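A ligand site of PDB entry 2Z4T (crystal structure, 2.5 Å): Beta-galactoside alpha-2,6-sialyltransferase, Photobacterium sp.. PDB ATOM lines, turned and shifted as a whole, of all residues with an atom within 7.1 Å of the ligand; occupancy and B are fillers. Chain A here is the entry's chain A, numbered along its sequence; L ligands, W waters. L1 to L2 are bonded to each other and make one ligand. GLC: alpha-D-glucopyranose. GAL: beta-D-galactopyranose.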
ATOM      1  N   ASP A 122     -21.266   0.201 -18.488  1.00  0.00           N
ATOM      2  CA  ASP A 122     -21.916   0.983 -17.464  1.00  0.00           C
ATOM      3  C   ASP A 122     -21.011   1.182 -16.248  1.00  0.00           C
ATOM      4  O   ASP A 122     -20.240   0.291 -15.871  1.00  0.00           O
ATOM      5  CB  ASP A 122     -23.241   0.318 -17.036  1.00  0.00           C
ATOM      6  CG  ASP A 122     -23.913   1.047 -15.894  1.00  0.00           C
ATOM      7  OD1 ASP A 122     -24.063   2.298 -15.978  1.00  0.00           O
ATOM      8  OD2 ASP A 122     -24.281   0.404 -14.902  1.00  0.00           O
ATOM      9  N   HIS A 123     -21.148   2.330 -15.613  1.00  0.00           N
ATOM     10  CA  HIS A 123     -20.318   2.672 -14.468  1.00  0.00           C
ATOM     11  C   HIS A 123     -21.187   2.701 -13.223  1.00  0.00           C
ATOM     12  O   HIS A 123     -20.657   2.776 -12.108  1.00  0.00           O
ATOM     13  CB  HIS A 123     -19.715   4.071 -14.665  1.00  0.00           C
ATOM     14  CG  HIS A 123     -20.741   5.153 -14.610  1.00  0.00           C
ATOM     15  ND1 HIS A 123     -21.605   5.412 -15.665  1.00  0.00           N
ATOM     16  CD2 HIS A 123     -21.090   6.012 -13.625  1.00  0.00           C
ATOM     17  CE1 HIS A 123     -22.424   6.391 -15.335  1.00  0.00           C
ATOM     18  NE2 HIS A 123     -22.140   6.769 -14.094  1.00  0.00           N
ATOM     19  N   ALA A 124     -22.510   2.657 -13.407  1.00  0.00           N
ATOM     20  CA  ALA A 124     -23.469   2.840 -12.314  1.00  0.00           C
ATOM     21  C   ALA A 124     -23.917   1.498 -11.736  1.00  0.00           C
ATOM     22  O   ALA A 124     -23.100   0.575 -11.654  1.00  0.00           O
ATOM     23  CB  ALA A 124     -24.647   3.662 -12.769  1.00  0.00           C
ATOM     24  N   SER A 125     -25.184   1.369 -11.315  1.00  0.00           N
ATOM     25  CA  SER A 125     -25.660   0.120 -10.674  1.00  0.00           C
ATOM     26  C   SER A 125     -26.770  -0.559 -11.446  1.00  0.00           C
ATOM     27  O   SER A 125     -26.690  -1.751 -11.754  1.00  0.00           O
ATOM     28  CB  SER A 125     -26.137   0.358  -9.239  1.00  0.00           C
ATOM     29  OG  SER A 125     -25.146   1.004  -8.470  1.00  0.00           O
ATOM     30  N   GLY A 152     -18.286  -0.719 -13.665  1.00  0.00           N
ATOM     31  CA  GLY A 152     -17.697  -0.119 -12.480  1.00  0.00           C
ATOM     32  C   GLY A 152     -17.952  -0.882 -11.185  1.00  0.00           C
ATOM     33  O   GLY A 152     -17.091  -0.933 -10.331  1.00  0.00           O
ATOM     34  N   ARG A 153     -19.126  -1.484 -11.054  1.00  0.00           N
ATOM     35  CA  ARG A 153     -19.608  -1.862  -9.706  1.00  0.00           C
ATOM     36  C   ARG A 153     -19.833  -3.355  -9.521  1.00  0.00           C
ATOM     37  O   ARG A 153     -20.254  -3.778  -8.445  1.00  0.00           O
ATOM     38  CB  ARG A 153     -20.873  -1.072  -9.347  1.00  0.00           C
ATOM     39  CG  ARG A 153     -20.661   0.425  -9.421  1.00  0.00           C
ATOM     40  CD  ARG A 153     -21.228   1.156  -8.238  1.00  0.00           C
ATOM     41  NE  ARG A 153     -20.671   2.507  -8.174  1.00  0.00           N
ATOM     42  CZ  ARG A 153     -19.754   2.928  -7.297  1.00  0.00           C
ATOM     43  NH1 ARG A 153     -19.259   2.099  -6.368  1.00  0.00           N
ATOM     44  NH2 ARG A 153     -19.340   4.184  -7.350  1.00  0.00           N
ATOM     45  N   ASN A 173     -12.817   7.588 -17.033  1.00  0.00           N
ATOM     46  CA  ASN A 173     -13.798   8.652 -16.820  1.00  0.00           C
ATOM     47  C   ASN A 173     -15.231   8.106 -16.923  1.00  0.00           C
ATOM     48  O   ASN A 173     -16.119   8.773 -17.494  1.00  0.00           O
ATOM     49  CB  ASN A 173     -13.590   9.803 -17.821  1.00  0.00           C
ATOM     50  CG  ASN A 173     -12.177  10.369 -17.785  1.00  0.00           C
ATOM     51  OD1 ASN A 173     -11.644  10.649 -16.710  1.00  0.00           O
ATOM     52  ND2 ASN A 173     -11.564  10.551 -18.971  1.00  0.00           N
ATOM     53  N   ASN A 174     -15.428   6.890 -16.415  1.00  0.00           N
ATOM     54  CA  ASN A 174     -16.737   6.231 -16.381  1.00  0.00           C
ATOM     55  C   ASN A 174     -17.302   5.766 -17.695  1.00  0.00           C
ATOM     56  O   ASN A 174     -18.465   5.342 -17.760  1.00  0.00           O
ATOM     57  CB  ASN A 174     -17.757   7.153 -15.725  1.00  0.00           C
ATOM     58  CG  ASN A 174     -17.403   7.448 -14.286  1.00  0.00           C
ATOM     59  OD1 ASN A 174     -16.845   6.594 -13.596  1.00  0.00           O
ATOM     60  ND2 ASN A 174     -17.723   8.638 -13.828  1.00  0.00           N
ATOM     61  N   ASN A 201     -25.764   2.065 -20.309  1.00  0.00           N
ATOM     62  CA  ASN A 201     -26.348   3.152 -19.534  1.00  0.00           C
ATOM     63  C   ASN A 201     -26.957   4.201 -20.495  1.00  0.00           C
ATOM     64  O   ASN A 201     -26.281   4.668 -21.410  1.00  0.00           O
ATOM     65  CB  ASN A 201     -25.233   3.762 -18.652  1.00  0.00           C
ATOM     66  CG  ASN A 201     -25.709   4.903 -17.768  1.00  0.00           C
ATOM     67  OD1 ASN A 201     -26.182   5.943 -18.257  1.00  0.00           O
ATOM     68  ND2 ASN A 201     -25.539   4.742 -16.452  1.00  0.00           N
ATOM     69  N   ALA A 203     -28.412   7.478 -20.039  1.00  0.00           N
ATOM     70  CA  ALA A 203     -27.940   8.872 -19.897  1.00  0.00           C
ATOM     71  C   ALA A 203     -26.552   9.078 -20.459  1.00  0.00           C
ATOM     72  O   ALA A 203     -26.242  10.164 -20.955  1.00  0.00           O
ATOM     73  CB  ALA A 203     -27.982   9.334 -18.446  1.00  0.00           C
ATOM     74  N   HIS A 204     -25.724   8.029 -20.356  1.00  0.00           N
ATOM     75  CA  HIS A 204     -24.317   8.059 -20.801  1.00  0.00           C
ATOM     76  C   HIS A 204     -24.066   7.321 -22.128  1.00  0.00           C
ATOM     77  O   HIS A 204     -22.909   7.010 -22.431  1.00  0.00           O
ATOM     78  CB  HIS A 204     -23.426   7.443 -19.713  1.00  0.00           C
ATOM     79  CG  HIS A 204     -23.380   8.253 -18.450  1.00  0.00           C
ATOM     80  ND1 HIS A 204     -22.369   9.141 -18.180  1.00  0.00           N
ATOM     81  CD2 HIS A 204     -24.248   8.340 -17.409  1.00  0.00           C
ATOM     82  CE1 HIS A 204     -22.605   9.737 -17.020  1.00  0.00           C
ATOM     83  NE2 HIS A 204     -23.749   9.274 -16.543  1.00  0.00           N
ATOM     84  N   ASP A 232     -29.684   4.679 -16.123  1.00  0.00           N
ATOM     85  CA  ASP A 232     -28.844   4.877 -14.955  1.00  0.00           C
ATOM     86  C   ASP A 232     -29.710   4.739 -13.709  1.00  0.00           C
ATOM     87  O   ASP A 232     -29.322   4.080 -12.749  1.00  0.00           O
ATOM     88  CB  ASP A 232     -28.225   6.267 -15.035  1.00  0.00           C
ATOM     89  CG  ASP A 232     -27.175   6.495 -13.982  1.00  0.00           C
ATOM     90  OD1 ASP A 232     -27.517   6.576 -12.769  1.00  0.00           O
ATOM     91  OD2 ASP A 232     -25.990   6.604 -14.385  1.00  0.00           O
ATOM     92  N   GLY A 233     -30.889   5.355 -13.758  1.00  0.00           N
ATOM     93  CA  GLY A 233     -31.893   5.248 -12.724  1.00  0.00           C
ATOM     94  C   GLY A 233     -32.730   6.522 -12.758  1.00  0.00           C
ATOM     95  O   GLY A 233     -33.250   6.912 -13.789  1.00  0.00           O
ATOM     96  N   SER A 234     -32.831   7.199 -11.618  1.00  0.00           N
ATOM     97  CA  SER A 234     -33.637   8.404 -11.531  1.00  0.00           C
ATOM     98  C   SER A 234     -33.023   9.516 -12.384  1.00  0.00           C
ATOM     99  O   SER A 234     -33.743  10.386 -12.853  1.00  0.00           O
ATOM    100  CB  SER A 234     -33.789   8.829 -10.068  1.00  0.00           C
ATOM    101  OG  SER A 234     -32.549   9.221  -9.494  1.00  0.00           O
ATOM    102  N   ALA A 235     -31.717   9.448 -12.621  1.00  0.00           N
ATOM    103  CA  ALA A 235     -31.001  10.481 -13.399  1.00  0.00           C
ATOM    104  C   ALA A 235     -31.676  10.802 -14.712  1.00  0.00           C
ATOM    105  O   ALA A 235     -31.816  11.980 -15.053  1.00  0.00           O
ATOM    106  CB  ALA A 235     -29.544  10.094 -13.632  1.00  0.00           C
ATOM    107  N   VAL A 364     -23.473  10.844  -2.125  1.00  0.00           N
ATOM    108  CA  VAL A 364     -23.386  12.092  -2.878  1.00  0.00           C
ATOM    109  C   VAL A 364     -22.480  11.907  -4.072  1.00  0.00           C
ATOM    110  O   VAL A 364     -21.335  11.487  -3.908  1.00  0.00           O
ATOM    111  CB  VAL A 364     -22.686  13.232  -2.114  1.00  0.00           C
ATOM    112  CG1 VAL A 364     -23.474  14.528  -2.316  1.00  0.00           C
ATOM    113  CG2 VAL A 364     -22.407  12.894  -0.659  1.00  0.00           C
ATOM    114  N   TRP A 365     -22.971  12.265  -5.255  1.00  0.00           N
ATOM    115  CA  TRP A 365     -22.100  12.364  -6.435  1.00  0.00           C
ATOM    116  C   TRP A 365     -21.498  13.781  -6.533  1.00  0.00           C
ATOM    117  O   TRP A 365     -22.136  14.776  -6.162  1.00  0.00           O
ATOM    118  CB  TRP A 365     -22.866  12.019  -7.728  1.00  0.00           C
ATOM    119  CG  TRP A 365     -23.575  10.674  -7.732  1.00  0.00           C
ATOM    120  CD1 TRP A 365     -24.892  10.447  -8.036  1.00  0.00           C
ATOM    121  CD2 TRP A 365     -22.993   9.383  -7.468  1.00  0.00           C
ATOM    122  NE1 TRP A 365     -25.179   9.094  -7.953  1.00  0.00           N
ATOM    123  CE2 TRP A 365     -24.036   8.414  -7.612  1.00  0.00           C
ATOM    124  CE3 TRP A 365     -21.719   8.936  -7.106  1.00  0.00           C
ATOM    125  CZ2 TRP A 365     -23.833   7.042  -7.422  1.00  0.00           C
ATOM    126  CZ3 TRP A 365     -21.514   7.567  -6.902  1.00  0.00           C
ATOM    127  CH2 TRP A 365     -22.576   6.638  -7.060  1.00  0.00           C
ATOM    128  N   ALA A 366     -20.260  13.874  -7.015  1.00  0.00           N
ATOM    129  CA  ALA A 366     -19.595  15.175  -7.207  1.00  0.00           C
ATOM    130  C   ALA A 366     -19.734  16.106  -5.985  1.00  0.00           C
ATOM    131  O   ALA A 366     -19.964  17.306  -6.132  1.00  0.00           O
ATOM    132  CB  ALA A 366     -20.166  15.872  -8.461  1.00  0.00           C
ATOM    133  N   GLY A 367     -19.601  15.539  -4.784  1.00  0.00           N
ATOM    134  CA  GLY A 367     -19.708  16.321  -3.556  1.00  0.00           C
ATOM    135  C   GLY A 367     -19.033  15.668  -2.359  1.00  0.00           C
ATOM    136  O   GLY A 367     -19.601  15.647  -1.261  1.00  0.00           O
ATOM    137  N   ASN A 368     -17.816  15.169  -2.533  1.00  0.00           N
ATOM    138  CA  ASN A 368     -17.077  14.591  -1.407  1.00  0.00           C
ATOM    139  C   ASN A 368     -17.052  15.409  -0.114  1.00  0.00           C
ATOM    140  O   ASN A 368     -17.090  14.852   0.981  1.00  0.00           O
ATOM    141  CB  ASN A 368     -15.660  14.197  -1.830  1.00  0.00           C
ATOM    142  CG  ASN A 368     -15.633  12.913  -2.644  1.00  0.00           C
ATOM    143  OD1 ASN A 368     -16.676  12.269  -2.847  1.00  0.00           O
ATOM    144  ND2 ASN A 368     -14.462  12.536  -3.118  1.00  0.00           N
ATOM    145  N   HIS A 405     -26.356   2.056  -0.314  1.00  0.00           N
ATOM    146  CA  HIS A 405     -25.577   2.638  -1.441  1.00  0.00           C
ATOM    147  C   HIS A 405     -24.256   2.067  -1.940  1.00  0.00           C
ATOM    148  O   HIS A 405     -23.244   2.158  -1.268  1.00  0.00           O
ATOM    149  CB  HIS A 405     -25.710   4.156  -1.624  1.00  0.00           C
ATOM    150  CG  HIS A 405     -25.944   4.565  -3.045  1.00  0.00           C
ATOM    151  ND1 HIS A 405     -24.976   4.460  -4.032  1.00  0.00           N
ATOM    152  CD2 HIS A 405     -27.054   5.043  -3.676  1.00  0.00           C
ATOM    153  CE1 HIS A 405     -25.471   4.860  -5.187  1.00  0.00           C
ATOM    154  NE2 HIS A 405     -26.729   5.234  -5.000  1.00  0.00           N
ATOM    155  N   GLY A 407     -22.186   3.069  -4.080  1.00  0.00           N
ATOM    156  CA  GLY A 407     -21.164   4.102  -4.101  1.00  0.00           C
ATOM    157  C   GLY A 407     -21.040   4.927  -2.825  1.00  0.00           C
ATOM    158  O   GLY A 407     -20.533   6.045  -2.854  1.00  0.00           O
ATOM    159  N   SER A 450     -33.547   5.417  -6.872  1.00  0.00           N
ATOM    160  CA  SER A 450     -34.099   4.647  -7.964  1.00  0.00           C
ATOM    161  C   SER A 450     -34.739   3.337  -7.503  1.00  0.00           C
ATOM    162  O   SER A 450     -35.675   2.823  -8.128  1.00  0.00           O
ATOM    163  CB  SER A 450     -33.021   4.343  -9.005  1.00  0.00           C
ATOM    164  OG  SER A 450     -32.286   5.506  -9.332  1.00  0.00           O
HETATM  165  C1  GLC L   1     -17.227   8.467  -9.317  1.00  0.00           C
HETATM  166  C2  GLC L   1     -18.385   7.462  -9.222  1.00  0.00           C
HETATM  167  C3  GLC L   1     -19.378   7.768 -10.340  1.00  0.00           C
HETATM  168  C4  GLC L   1     -19.820   9.249 -10.369  1.00  0.00           C
HETATM  169  C5  GLC L   1     -18.559  10.164 -10.314  1.00  0.00           C
HETATM  170  C6  GLC L   1     -18.715  11.692 -10.261  1.00  0.00           C
HETATM  171  O1  GLC L   1     -16.582   8.388 -10.588  1.00  0.00           O
HETATM  172  O2  GLC L   1     -17.956   6.132  -9.364  1.00  0.00           O
HETATM  173  O3  GLC L   1     -20.462   6.883 -10.246  1.00  0.00           O
HETATM  174  O4  GLC L   1     -20.559   9.452 -11.549  1.00  0.00           O
HETATM  175  O5  GLC L   1     -17.760   9.781  -9.198  1.00  0.00           O
HETATM  176  O6  GLC L   1     -20.042  12.183 -10.177  1.00  0.00           O
HETATM  177  C1  GAL L   2     -21.950   9.663 -11.456  1.00  0.00           C
HETATM  178  C2  GAL L   2     -22.353  10.403 -12.733  1.00  0.00           C
HETATM  179  C3  GAL L   2     -23.870  10.587 -12.746  1.00  0.00           C
HETATM  180  C4  GAL L   2     -24.579   9.249 -12.494  1.00  0.00           C
HETATM  181  C5  GAL L   2     -24.029   8.542 -11.263  1.00  0.00           C
HETATM  182  C6  GAL L   2     -24.558   7.106 -11.099  1.00  0.00           C
HETATM  183  O2  GAL L   2     -21.673  11.649 -12.805  1.00  0.00           O
HETATM  184  O3  GAL L   2     -24.288  11.139 -13.992  1.00  0.00           O
HETATM  185  O4  GAL L   2     -24.423   8.434 -13.649  1.00  0.00           O
HETATM  186  O5  GAL L   2     -22.626   8.438 -11.375  1.00  0.00           O
HETATM  187  O6  GAL L   2     -25.940   7.070 -10.820  1.00  0.00           O
HETATM  188  O   HOH W   1     -26.639  12.281 -13.711  1.00  0.00           O
HETATM  189  O   HOH W   2     -19.441  10.874 -14.744  1.00  0.00           O
HETATM  190  O   HOH W   3     -14.167   9.632  -9.674  1.00  0.00           O
HETATM  191  O   HOH W   4     -19.130  11.012  -6.697  1.00  0.00           O
HETATM  192  O   HOH W   5     -15.277   6.858  -7.179  1.00  0.00           O
HETATM  193  O   HOH W   6     -26.647   5.012  -9.274  1.00  0.00           O
HETATM  194  O   HOH W   7     -18.236   3.631 -10.953  1.00  0.00           O
HETATM  195  O   HOH W   8     -21.895   4.473  -9.683  1.00  0.00           O
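Water W8 lies within hydrogen-bond range of NE of Arg 153 (2.8 Å), O3 of GLC L1 (2.9 Å) and O of His 123 (3.2 Å). Water W7 bridges the backbone carbonyl oxygen of His 123 (2.8 Å) and an oxygen (O2) of GLC L1 (3.0 Å). Water W2 bridges the side-chain amide nitrogen (ND2) of Asn 174 (3.0 Å) and an oxygen (O2) of GAL L2 (3.1 Å). Water W4 lies within hydrogen-bond range of N of Ala 366 (3.1 Å) and O5 of GLC L1 (3.1 Å).
The side-chain carboxylate (OD2) of Asp 232 sits at hydrogen-bond distance from an oxygen (O4) of GAL L2, at 2.5 Å. NE2 of His 123 sits at hydrogen-bond distance from O4 of GAL L2, 2.9 Å away. NE2 of His 204 is in hydrogen-bond range of O4 of GAL L2 (3.1 Å). NH2 of Arg 153 sits at hydrogen-bond distance from O2 of GLC L1 (3.1 Å). ND2 of Asn 174 is in hydrogen-bond range of O1 of GLC L1.
The side-chain carboxylate (OD2) of Asp 232 lies within hydrogen-bond range of the side-chain amide nitrogen (ND2) of Asn 201 (2.8 Å). The backbone NH of His 204 sits at hydrogen-bond distance from the side-chain amide oxygen of Asn 201. The backbone NH (N) of Ala 124 sits at hydrogen-bond distance from the side-chain carboxylate (OD1) of Asp 122, at 3.0 Å.
Merely in contact with the ligand: Ala 124 (3.8 Å), Trp 365 (3.5 Å) and Ala 366 (3.6 Å). Hydrophobic or aromatic side chains that line the ligand: His 123, Ala 124, His 204 and Trp 365. Eight residues have an atom within 4 Å of the ligand: His 123, Ala 124, Arg 153, Asn 174, His 204, Asp 232, Trp 365 and Ala 366.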
